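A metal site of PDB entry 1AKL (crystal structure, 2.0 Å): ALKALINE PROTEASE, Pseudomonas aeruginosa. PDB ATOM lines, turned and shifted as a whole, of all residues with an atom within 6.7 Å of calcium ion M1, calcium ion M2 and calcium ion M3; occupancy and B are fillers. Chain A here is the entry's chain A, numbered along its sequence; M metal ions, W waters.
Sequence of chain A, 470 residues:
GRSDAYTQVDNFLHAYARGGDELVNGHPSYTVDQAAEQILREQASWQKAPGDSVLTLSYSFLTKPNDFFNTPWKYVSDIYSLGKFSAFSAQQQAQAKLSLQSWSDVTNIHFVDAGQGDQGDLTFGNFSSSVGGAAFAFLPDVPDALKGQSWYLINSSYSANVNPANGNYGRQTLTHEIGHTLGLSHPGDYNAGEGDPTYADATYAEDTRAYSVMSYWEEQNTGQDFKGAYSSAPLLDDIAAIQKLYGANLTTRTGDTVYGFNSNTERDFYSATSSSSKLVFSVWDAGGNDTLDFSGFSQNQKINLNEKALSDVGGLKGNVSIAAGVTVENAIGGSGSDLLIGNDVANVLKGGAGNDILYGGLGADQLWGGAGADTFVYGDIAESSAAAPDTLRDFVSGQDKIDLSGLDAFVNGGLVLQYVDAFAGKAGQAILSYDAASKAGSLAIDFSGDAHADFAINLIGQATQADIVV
N of Gly 370 sits at hydrogen-bond distance from OD2 of Asp 394.
The side-chain carboxylate (OD1) of Asp 338 is in hydrogen-bond range of the backbone NH (N) of Gln 301.
The side-chain amide nitrogen of Gln 301 sits close to the backbone NH of Gly 334 (3.5 Å).
The side-chain carboxylate of Asp 400 is in hydrogen-bond range of the backbone NH of Val 396.
The backbone carbonyl oxygen of Trp 368 sits at hydrogen-bond distance from the backbone NH of Gly 351 (2.9 Å).
N of Gly 369 sits at hydrogen-bond distance from OD1 of Asp 394 (3.0 Å).
Within 4 Å of calcium ion M3: Gly 370, Ala 371, Gly 372, Asp 374, Gln 399 and Asp 400.
The nearest printed residue that does not touch calcium ion M3 is Ala 373 (4.5 Å).
Water W1 lies within hydrogen-bond range of the side-chain carboxylate of Asp 400 and the backbone carbonyl oxygen of Asp 394.
Calcium ion M2 is bound by the backbone carbonyl oxygen (O) of Gly 369 (2.2 Å), the backbone carbonyl oxygen (O) of Ala 371 (2.3 Å), the backbone carbonyl oxygen (O) of Gly 352 (2.3 Å), the backbone carbonyl oxygen (O) of Gly 354 (2.4 Å), the side-chain carboxylate (OD1) of Asp 374 (2.5 Å) and the side-chain carboxylate (OD2) of Asp 356 (2.5 Å).
Slightly farther from calcium ion M2 lies OD2 of Asp 374 (3.1 Å).
Calcium ion M3 is bound by O of Gly 372 (2.2 Å), water W1 (2.4 Å), O of Gly 370 (2.5 Å), OD1 of Asp 400 (2.7 Å), OD2 of Asp 374 (2.8 Å) and OE1 of Gln 399 (2.8 Å).
Eight residues have an atom within 4 Å of calcium ion M2: Gly 352, Ala 353, Gly 354, Asp 356, Gly 369, Gly 370, Ala 371 and Asp 374.
The nearest printed residue that does not touch calcium ion M2 is Gly 351 (4.2 Å).
Merely in contact with calcium ion M1: Ser 335.
Of the 30 residues printed, 8 come within 4 Å of calcium ion M1.
The nearest printed residue that does not touch calcium ion M1 is Gly 354 (4.4 Å).
Calcium ion M1 is bound by O of Gly 334 (2.2 Å), O of Gly 336 (2.2 Å), O of Ala 353 (2.3 Å), O of Gly 351 (2.3 Å), OD1 of Asp 356 (2.5 Å) and OD2 of Asp 338 (2.7 Å).
Calcium ion M1 has six donor atoms within binding distance.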
ATOM      1  N   GLN A 299      -6.061  23.907  -1.981  1.00  0.00           N
ATOM      2  CA  GLN A 299      -6.337  25.034  -1.101  1.00  0.00           C
ATOM      3  C   GLN A 299      -7.578  25.791  -1.515  1.00  0.00           C
ATOM      4  O   GLN A 299      -8.048  25.665  -2.646  1.00  0.00           O
ATOM      5  CB  GLN A 299      -5.168  26.012  -1.106  1.00  0.00           C
ATOM      6  CG  GLN A 299      -3.884  25.451  -0.601  1.00  0.00           C
ATOM      7  CD  GLN A 299      -3.072  24.824  -1.674  1.00  0.00           C
ATOM      8  OE1 GLN A 299      -3.571  24.484  -2.739  1.00  0.00           O
ATOM      9  NE2 GLN A 299      -1.792  24.668  -1.410  1.00  0.00           N
ATOM     10  N   GLN A 301      -9.291  28.761  -2.913  1.00  0.00           N
ATOM     11  CA  GLN A 301      -8.819  29.796  -3.821  1.00  0.00           C
ATOM     12  C   GLN A 301      -9.884  30.826  -4.153  1.00  0.00           C
ATOM     13  O   GLN A 301     -11.068  30.557  -3.994  1.00  0.00           O
ATOM     14  CB  GLN A 301      -8.360  29.131  -5.117  1.00  0.00           C
ATOM     15  CG  GLN A 301      -7.499  27.911  -4.895  1.00  0.00           C
ATOM     16  CD  GLN A 301      -7.046  27.303  -6.204  1.00  0.00           C
ATOM     17  OE1 GLN A 301      -6.110  27.811  -6.833  1.00  0.00           O
ATOM     18  NE2 GLN A 301      -7.692  26.244  -6.630  1.00  0.00           N
ATOM     19  N   GLY A 333     -11.765  25.850 -10.734  1.00  0.00           N
ATOM     20  CA  GLY A 333     -11.270  25.804  -9.378  1.00  0.00           C
ATOM     21  C   GLY A 333     -10.788  24.414  -9.038  1.00  0.00           C
ATOM     22  O   GLY A 333     -10.905  23.502  -9.857  1.00  0.00           O
ATOM     23  N   GLY A 334     -10.266  24.240  -7.833  1.00  0.00           N
ATOM     24  CA  GLY A 334      -9.778  22.941  -7.396  1.00  0.00           C
ATOM     25  C   GLY A 334     -10.711  22.290  -6.395  1.00  0.00           C
ATOM     26  O   GLY A 334     -11.848  22.713  -6.232  1.00  0.00           O
ATOM     27  N   SER A 335     -10.213  21.307  -5.652  1.00  0.00           N
ATOM     28  CA  SER A 335     -11.045  20.613  -4.682  1.00  0.00           C
ATOM     29  C   SER A 335     -11.353  21.378  -3.400  1.00  0.00           C
ATOM     30  O   SER A 335     -12.129  20.916  -2.564  1.00  0.00           O
ATOM     31  CB  SER A 335     -10.450  19.240  -4.371  1.00  0.00           C
ATOM     32  OG  SER A 335      -9.117  19.345  -3.919  1.00  0.00           O
ATOM     33  N   GLY A 336     -10.762  22.564  -3.247  1.00  0.00           N
ATOM     34  CA  GLY A 336     -11.031  23.351  -2.058  1.00  0.00           C
ATOM     35  C   GLY A 336     -12.300  24.150  -2.296  1.00  0.00           C
ATOM     36  O   GLY A 336     -12.857  24.125  -3.406  1.00  0.00           O
ATOM     37  N   SER A 337     -12.777  24.825  -1.266  1.00  0.00           N
ATOM     38  CA  SER A 337     -13.972  25.647  -1.394  1.00  0.00           C
ATOM     39  C   SER A 337     -13.521  26.979  -1.972  1.00  0.00           C
ATOM     40  O   SER A 337     -12.883  27.782  -1.293  1.00  0.00           O
ATOM     41  CB  SER A 337     -14.656  25.815  -0.038  1.00  0.00           C
ATOM     42  OG  SER A 337     -15.183  24.568   0.413  1.00  0.00           O
ATOM     43  N   ASP A 338     -13.848  27.204  -3.243  1.00  0.00           N
ATOM     44  CA  ASP A 338     -13.420  28.394  -3.972  1.00  0.00           C
ATOM     45  C   ASP A 338     -14.467  29.473  -4.179  1.00  0.00           C
ATOM     46  O   ASP A 338     -15.668  29.252  -4.013  1.00  0.00           O
ATOM     47  CB  ASP A 338     -12.895  27.989  -5.342  1.00  0.00           C
ATOM     48  CG  ASP A 338     -11.967  26.804  -5.290  1.00  0.00           C
ATOM     49  OD1 ASP A 338     -11.128  26.729  -4.363  1.00  0.00           O
ATOM     50  OD2 ASP A 338     -12.091  25.927  -6.173  1.00  0.00           O
ATOM     51  N   LEU A 340     -15.308  31.953  -7.351  1.00  0.00           N
ATOM     52  CA  LEU A 340     -14.984  32.270  -8.725  1.00  0.00           C
ATOM     53  C   LEU A 340     -15.834  33.391  -9.241  1.00  0.00           C
ATOM     54  O   LEU A 340     -17.041  33.240  -9.351  1.00  0.00           O
ATOM     55  CB  LEU A 340     -15.171  31.050  -9.622  1.00  0.00           C
ATOM     56  CG  LEU A 340     -14.257  29.825  -9.493  1.00  0.00           C
ATOM     57  CD1 LEU A 340     -14.733  28.927  -8.381  1.00  0.00           C
ATOM     58  CD2 LEU A 340     -14.271  29.058 -10.801  1.00  0.00           C
ATOM     59  N   LYS A 350     -16.071  26.656 -13.344  1.00  0.00           N
ATOM     60  CA  LYS A 350     -16.242  25.321 -12.803  1.00  0.00           C
ATOM     61  C   LYS A 350     -15.650  25.280 -11.414  1.00  0.00           C
ATOM     62  O   LYS A 350     -14.450  25.430 -11.248  1.00  0.00           O
ATOM     63  CB  LYS A 350     -15.580  24.283 -13.697  1.00  0.00           C
ATOM     64  CG  LYS A 350     -16.205  24.182 -15.074  1.00  0.00           C
ATOM     65  CD  LYS A 350     -15.594  23.057 -15.870  1.00  0.00           C
ATOM     66  CE  LYS A 350     -16.353  22.815 -17.162  1.00  0.00           C
ATOM     67  NZ  LYS A 350     -15.686  21.784 -18.019  1.00  0.00           N
ATOM     68  N   GLY A 351     -16.481  25.071 -10.411  1.00  0.00           N
ATOM     69  CA  GLY A 351     -15.980  25.062  -9.060  1.00  0.00           C
ATOM     70  C   GLY A 351     -15.276  23.808  -8.610  1.00  0.00           C
ATOM     71  O   GLY A 351     -14.575  23.833  -7.590  1.00  0.00           O
ATOM     72  N   GLY A 352     -15.503  22.706  -9.322  1.00  0.00           N
ATOM     73  CA  GLY A 352     -14.880  21.449  -8.945  1.00  0.00           C
ATOM     74  C   GLY A 352     -15.409  21.011  -7.594  1.00  0.00           C
ATOM     75  O   GLY A 352     -16.448  21.499  -7.145  1.00  0.00           O
ATOM     76  N   ALA A 353     -14.703  20.116  -6.908  1.00  0.00           N
ATOM     77  CA  ALA A 353     -15.152  19.661  -5.604  1.00  0.00           C
ATOM     78  C   ALA A 353     -15.173  20.822  -4.607  1.00  0.00           C
ATOM     79  O   ALA A 353     -14.783  21.941  -4.958  1.00  0.00           O
ATOM     80  CB  ALA A 353     -14.270  18.537  -5.091  1.00  0.00           C
ATOM     81  N   GLY A 354     -15.628  20.568  -3.396  1.00  0.00           N
ATOM     82  CA  GLY A 354     -15.714  21.620  -2.410  1.00  0.00           C
ATOM     83  C   GLY A 354     -16.935  22.497  -2.625  1.00  0.00           C
ATOM     84  O   GLY A 354     -17.551  22.506  -3.712  1.00  0.00           O
ATOM     85  N   ASN A 355     -17.254  23.280  -1.600  1.00  0.00           N
ATOM     86  CA  ASN A 355     -18.408  24.170  -1.642  1.00  0.00           C
ATOM     87  C   ASN A 355     -18.021  25.542  -2.162  1.00  0.00           C
ATOM     88  O   ASN A 355     -17.517  26.389  -1.433  1.00  0.00           O
ATOM     89  CB  ASN A 355     -19.026  24.267  -0.245  1.00  0.00           C
ATOM     90  CG  ASN A 355     -19.545  22.920   0.246  1.00  0.00           C
ATOM     91  OD1 ASN A 355     -19.734  21.983  -0.541  1.00  0.00           O
ATOM     92  ND2 ASN A 355     -19.767  22.811   1.548  1.00  0.00           N
ATOM     93  N   ASP A 356     -18.307  25.765  -3.436  1.00  0.00           N
ATOM     94  CA  ASP A 356     -17.940  26.995  -4.120  1.00  0.00           C
ATOM     95  C   ASP A 356     -19.025  28.039  -4.233  1.00  0.00           C
ATOM     96  O   ASP A 356     -20.214  27.743  -4.162  1.00  0.00           O
ATOM     97  CB  ASP A 356     -17.432  26.661  -5.519  1.00  0.00           C
ATOM     98  CG  ASP A 356     -16.532  25.451  -5.534  1.00  0.00           C
ATOM     99  OD1 ASP A 356     -15.422  25.515  -4.976  1.00  0.00           O
ATOM    100  OD2 ASP A 356     -16.941  24.428  -6.101  1.00  0.00           O
ATOM    101  N   LEU A 358     -20.078  30.772  -6.972  1.00  0.00           N
ATOM    102  CA  LEU A 358     -19.897  31.184  -8.360  1.00  0.00           C
ATOM    103  C   LEU A 358     -20.677  32.467  -8.647  1.00  0.00           C
ATOM    104  O   LEU A 358     -21.864  32.553  -8.361  1.00  0.00           O
ATOM    105  CB  LEU A 358     -20.399  30.093  -9.319  1.00  0.00           C
ATOM    106  CG  LEU A 358     -19.870  28.646  -9.360  1.00  0.00           C
ATOM    107  CD1 LEU A 358     -18.585  28.577 -10.111  1.00  0.00           C
ATOM    108  CD2 LEU A 358     -19.767  28.031  -7.988  1.00  0.00           C
ATOM    109  N   TRP A 368     -20.891  25.759 -13.509  1.00  0.00           N
ATOM    110  CA  TRP A 368     -20.850  24.369 -13.059  1.00  0.00           C
ATOM    111  C   TRP A 368     -20.324  24.405 -11.632  1.00  0.00           C
ATOM    112  O   TRP A 368     -19.212  24.819 -11.388  1.00  0.00           O
ATOM    113  CB  TRP A 368     -19.887  23.536 -13.901  1.00  0.00           C
ATOM    114  CG  TRP A 368     -20.141  23.483 -15.367  1.00  0.00           C
ATOM    115  CD1 TRP A 368     -19.973  24.504 -16.269  1.00  0.00           C
ATOM    116  CD2 TRP A 368     -20.551  22.342 -16.116  1.00  0.00           C
ATOM    117  NE1 TRP A 368     -20.247  24.051 -17.546  1.00  0.00           N
ATOM    118  CE2 TRP A 368     -20.605  22.735 -17.477  1.00  0.00           C
ATOM    119  CE3 TRP A 368     -20.882  21.024 -15.773  1.00  0.00           C
ATOM    120  CZ2 TRP A 368     -20.976  21.856 -18.490  1.00  0.00           C
ATOM    121  CZ3 TRP A 368     -21.254  20.145 -16.786  1.00  0.00           C
ATOM    122  CH2 TRP A 368     -21.294  20.576 -18.136  1.00  0.00           C
ATOM    123  N   GLY A 369     -21.115  23.945 -10.677  1.00  0.00           N
ATOM    124  CA  GLY A 369     -20.639  23.960  -9.314  1.00  0.00           C
ATOM    125  C   GLY A 369     -19.855  22.720  -8.953  1.00  0.00           C
ATOM    126  O   GLY A 369     -19.051  22.733  -8.006  1.00  0.00           O
ATOM    127  N   GLY A 370     -20.115  21.635  -9.661  1.00  0.00           N
ATOM    128  CA  GLY A 370     -19.441  20.380  -9.371  1.00  0.00           C
ATOM    129  C   GLY A 370     -19.905  19.793  -8.046  1.00  0.00           C
ATOM    130  O   GLY A 370     -20.905  20.234  -7.459  1.00  0.00           O
ATOM    131  N   ALA A 371     -19.153  18.816  -7.550  1.00  0.00           N
ATOM    132  CA  ALA A 371     -19.458  18.161  -6.286  1.00  0.00           C
ATOM    133  C   ALA A 371     -19.599  19.210  -5.186  1.00  0.00           C
ATOM    134  O   ALA A 371     -19.093  20.334  -5.331  1.00  0.00           O
ATOM    135  CB  ALA A 371     -18.352  17.187  -5.940  1.00  0.00           C
ATOM    136  N   GLY A 372     -20.309  18.874  -4.117  1.00  0.00           N
ATOM    137  CA  GLY A 372     -20.485  19.796  -3.005  1.00  0.00           C
ATOM    138  C   GLY A 372     -21.639  20.766  -3.136  1.00  0.00           C
ATOM    139  O   GLY A 372     -22.204  20.940  -4.239  1.00  0.00           O
ATOM    140  N   ALA A 373     -21.960  21.426  -2.038  1.00  0.00           N
ATOM    141  CA  ALA A 373     -23.037  22.396  -1.968  1.00  0.00           C
ATOM    142  C   ALA A 373     -22.492  23.738  -2.420  1.00  0.00           C
ATOM    143  O   ALA A 373     -21.804  24.411  -1.675  1.00  0.00           O
ATOM    144  CB  ALA A 373     -23.547  22.501  -0.550  1.00  0.00           C
ATOM    145  N   ASP A 374     -22.859  24.128  -3.633  1.00  0.00           N
ATOM    146  CA  ASP A 374     -22.367  25.373  -4.202  1.00  0.00           C
ATOM    147  C   ASP A 374     -23.441  26.431  -4.256  1.00  0.00           C
ATOM    148  O   ASP A 374     -24.622  26.097  -4.370  1.00  0.00           O
ATOM    149  CB  ASP A 374     -21.845  25.105  -5.617  1.00  0.00           C
ATOM    150  CG  ASP A 374     -20.934  23.912  -5.659  1.00  0.00           C
ATOM    151  OD1 ASP A 374     -19.894  23.920  -4.969  1.00  0.00           O
ATOM    152  OD2 ASP A 374     -21.294  22.933  -6.340  1.00  0.00           O
ATOM    153  N   PHE A 376     -24.776  29.965  -6.199  1.00  0.00           N
ATOM    154  CA  PHE A 376     -24.664  30.735  -7.425  1.00  0.00           C
ATOM    155  C   PHE A 376     -25.229  32.121  -7.112  1.00  0.00           C
ATOM    156  O   PHE A 376     -26.439  32.299  -6.989  1.00  0.00           O
ATOM    157  CB  PHE A 376     -25.422  30.040  -8.556  1.00  0.00           C
ATOM    158  CG  PHE A 376     -25.005  28.603  -8.775  1.00  0.00           C
ATOM    159  CD1 PHE A 376     -25.588  27.578  -8.044  1.00  0.00           C
ATOM    160  CD2 PHE A 376     -23.983  28.286  -9.668  1.00  0.00           C
ATOM    161  CE1 PHE A 376     -25.164  26.255  -8.201  1.00  0.00           C
ATOM    162  CE2 PHE A 376     -23.551  26.979  -9.823  1.00  0.00           C
ATOM    163  CZ  PHE A 376     -24.146  25.959  -9.086  1.00  0.00           C
ATOM    164  N   ASP A 394     -25.467  22.043 -13.854  1.00  0.00           N
ATOM    165  CA  ASP A 394     -25.437  20.864 -12.976  1.00  0.00           C
ATOM    166  C   ASP A 394     -26.044  21.121 -11.600  1.00  0.00           C
ATOM    167  O   ASP A 394     -25.472  20.736 -10.562  1.00  0.00           O
ATOM    168  CB  ASP A 394     -23.993  20.363 -12.834  1.00  0.00           C
ATOM    169  CG  ASP A 394     -23.102  21.320 -12.068  1.00  0.00           C
ATOM    170  OD1 ASP A 394     -23.507  22.479 -11.809  1.00  0.00           O
ATOM    171  OD2 ASP A 394     -21.992  20.896 -11.707  1.00  0.00           O
ATOM    172  N   PHE A 395     -27.211  21.773 -11.603  1.00  0.00           N
ATOM    173  CA  PHE A 395     -27.883  22.109 -10.360  1.00  0.00           C
ATOM    174  C   PHE A 395     -28.424  20.868  -9.654  1.00  0.00           C
ATOM    175  O   PHE A 395     -28.863  19.900 -10.280  1.00  0.00           O
ATOM    176  CB  PHE A 395     -29.004  23.115 -10.629  1.00  0.00           C
ATOM    177  CG  PHE A 395     -29.435  23.871  -9.412  1.00  0.00           C
ATOM    178  CD1 PHE A 395     -28.737  25.010  -9.005  1.00  0.00           C
ATOM    179  CD2 PHE A 395     -30.521  23.446  -8.648  1.00  0.00           C
ATOM    180  CE1 PHE A 395     -29.132  25.723  -7.863  1.00  0.00           C
ATOM    181  CE2 PHE A 395     -30.914  24.145  -7.507  1.00  0.00           C
ATOM    182  CZ  PHE A 395     -30.224  25.283  -7.115  1.00  0.00           C
ATOM    183  N   VAL A 396     -28.362  20.906  -8.334  1.00  0.00           N
ATOM    184  CA  VAL A 396     -28.826  19.809  -7.506  1.00  0.00           C
ATOM    185  C   VAL A 396     -29.647  20.384  -6.386  1.00  0.00           C
ATOM    186  O   VAL A 396     -29.112  20.909  -5.402  1.00  0.00           O
ATOM    187  CB  VAL A 396     -27.637  19.041  -6.913  1.00  0.00           C
ATOM    188  CG1 VAL A 396     -28.097  18.145  -5.771  1.00  0.00           C
ATOM    189  CG2 VAL A 396     -26.980  18.220  -7.998  1.00  0.00           C
ATOM    190  N   GLN A 399     -29.120  20.906  -2.374  1.00  0.00           N
ATOM    191  CA  GLN A 399     -27.680  20.903  -2.170  1.00  0.00           C
ATOM    192  C   GLN A 399     -27.137  22.259  -2.622  1.00  0.00           C
ATOM    193  O   GLN A 399     -26.450  22.939  -1.870  1.00  0.00           O
ATOM    194  CB  GLN A 399     -27.018  19.770  -2.960  1.00  0.00           C
ATOM    195  CG  GLN A 399     -25.569  19.513  -2.558  1.00  0.00           C
ATOM    196  CD  GLN A 399     -24.839  18.565  -3.518  1.00  0.00           C
ATOM    197  OE1 GLN A 399     -24.438  18.966  -4.630  1.00  0.00           O
ATOM    198  NE2 GLN A 399     -24.624  17.328  -3.084  1.00  0.00           N
ATOM    199  N   ASP A 400     -27.473  22.653  -3.845  1.00  0.00           N
ATOM    200  CA  ASP A 400     -27.037  23.926  -4.399  1.00  0.00           C
ATOM    201  C   ASP A 400     -28.085  25.002  -4.114  1.00  0.00           C
ATOM    202  O   ASP A 400     -29.273  24.697  -3.964  1.00  0.00           O
ATOM    203  CB  ASP A 400     -26.849  23.814  -5.920  1.00  0.00           C
ATOM    204  CG  ASP A 400     -25.831  22.757  -6.314  1.00  0.00           C
ATOM    205  OD1 ASP A 400     -25.068  22.260  -5.456  1.00  0.00           O
ATOM    206  OD2 ASP A 400     -25.797  22.445  -7.520  1.00  0.00           O
HETATM  207 CA    CA M   1     -13.601  23.845  -5.496  1.00  0.00          CA
HETATM  208 CA    CA M   2     -18.281  22.368  -5.987  1.00  0.00          CA
HETATM  209 CA    CA M   3     -23.016  20.772  -6.312  1.00  0.00          CA
HETATM  210  O   HOH W   1     -23.444  21.885  -8.388  1.00  0.00           O
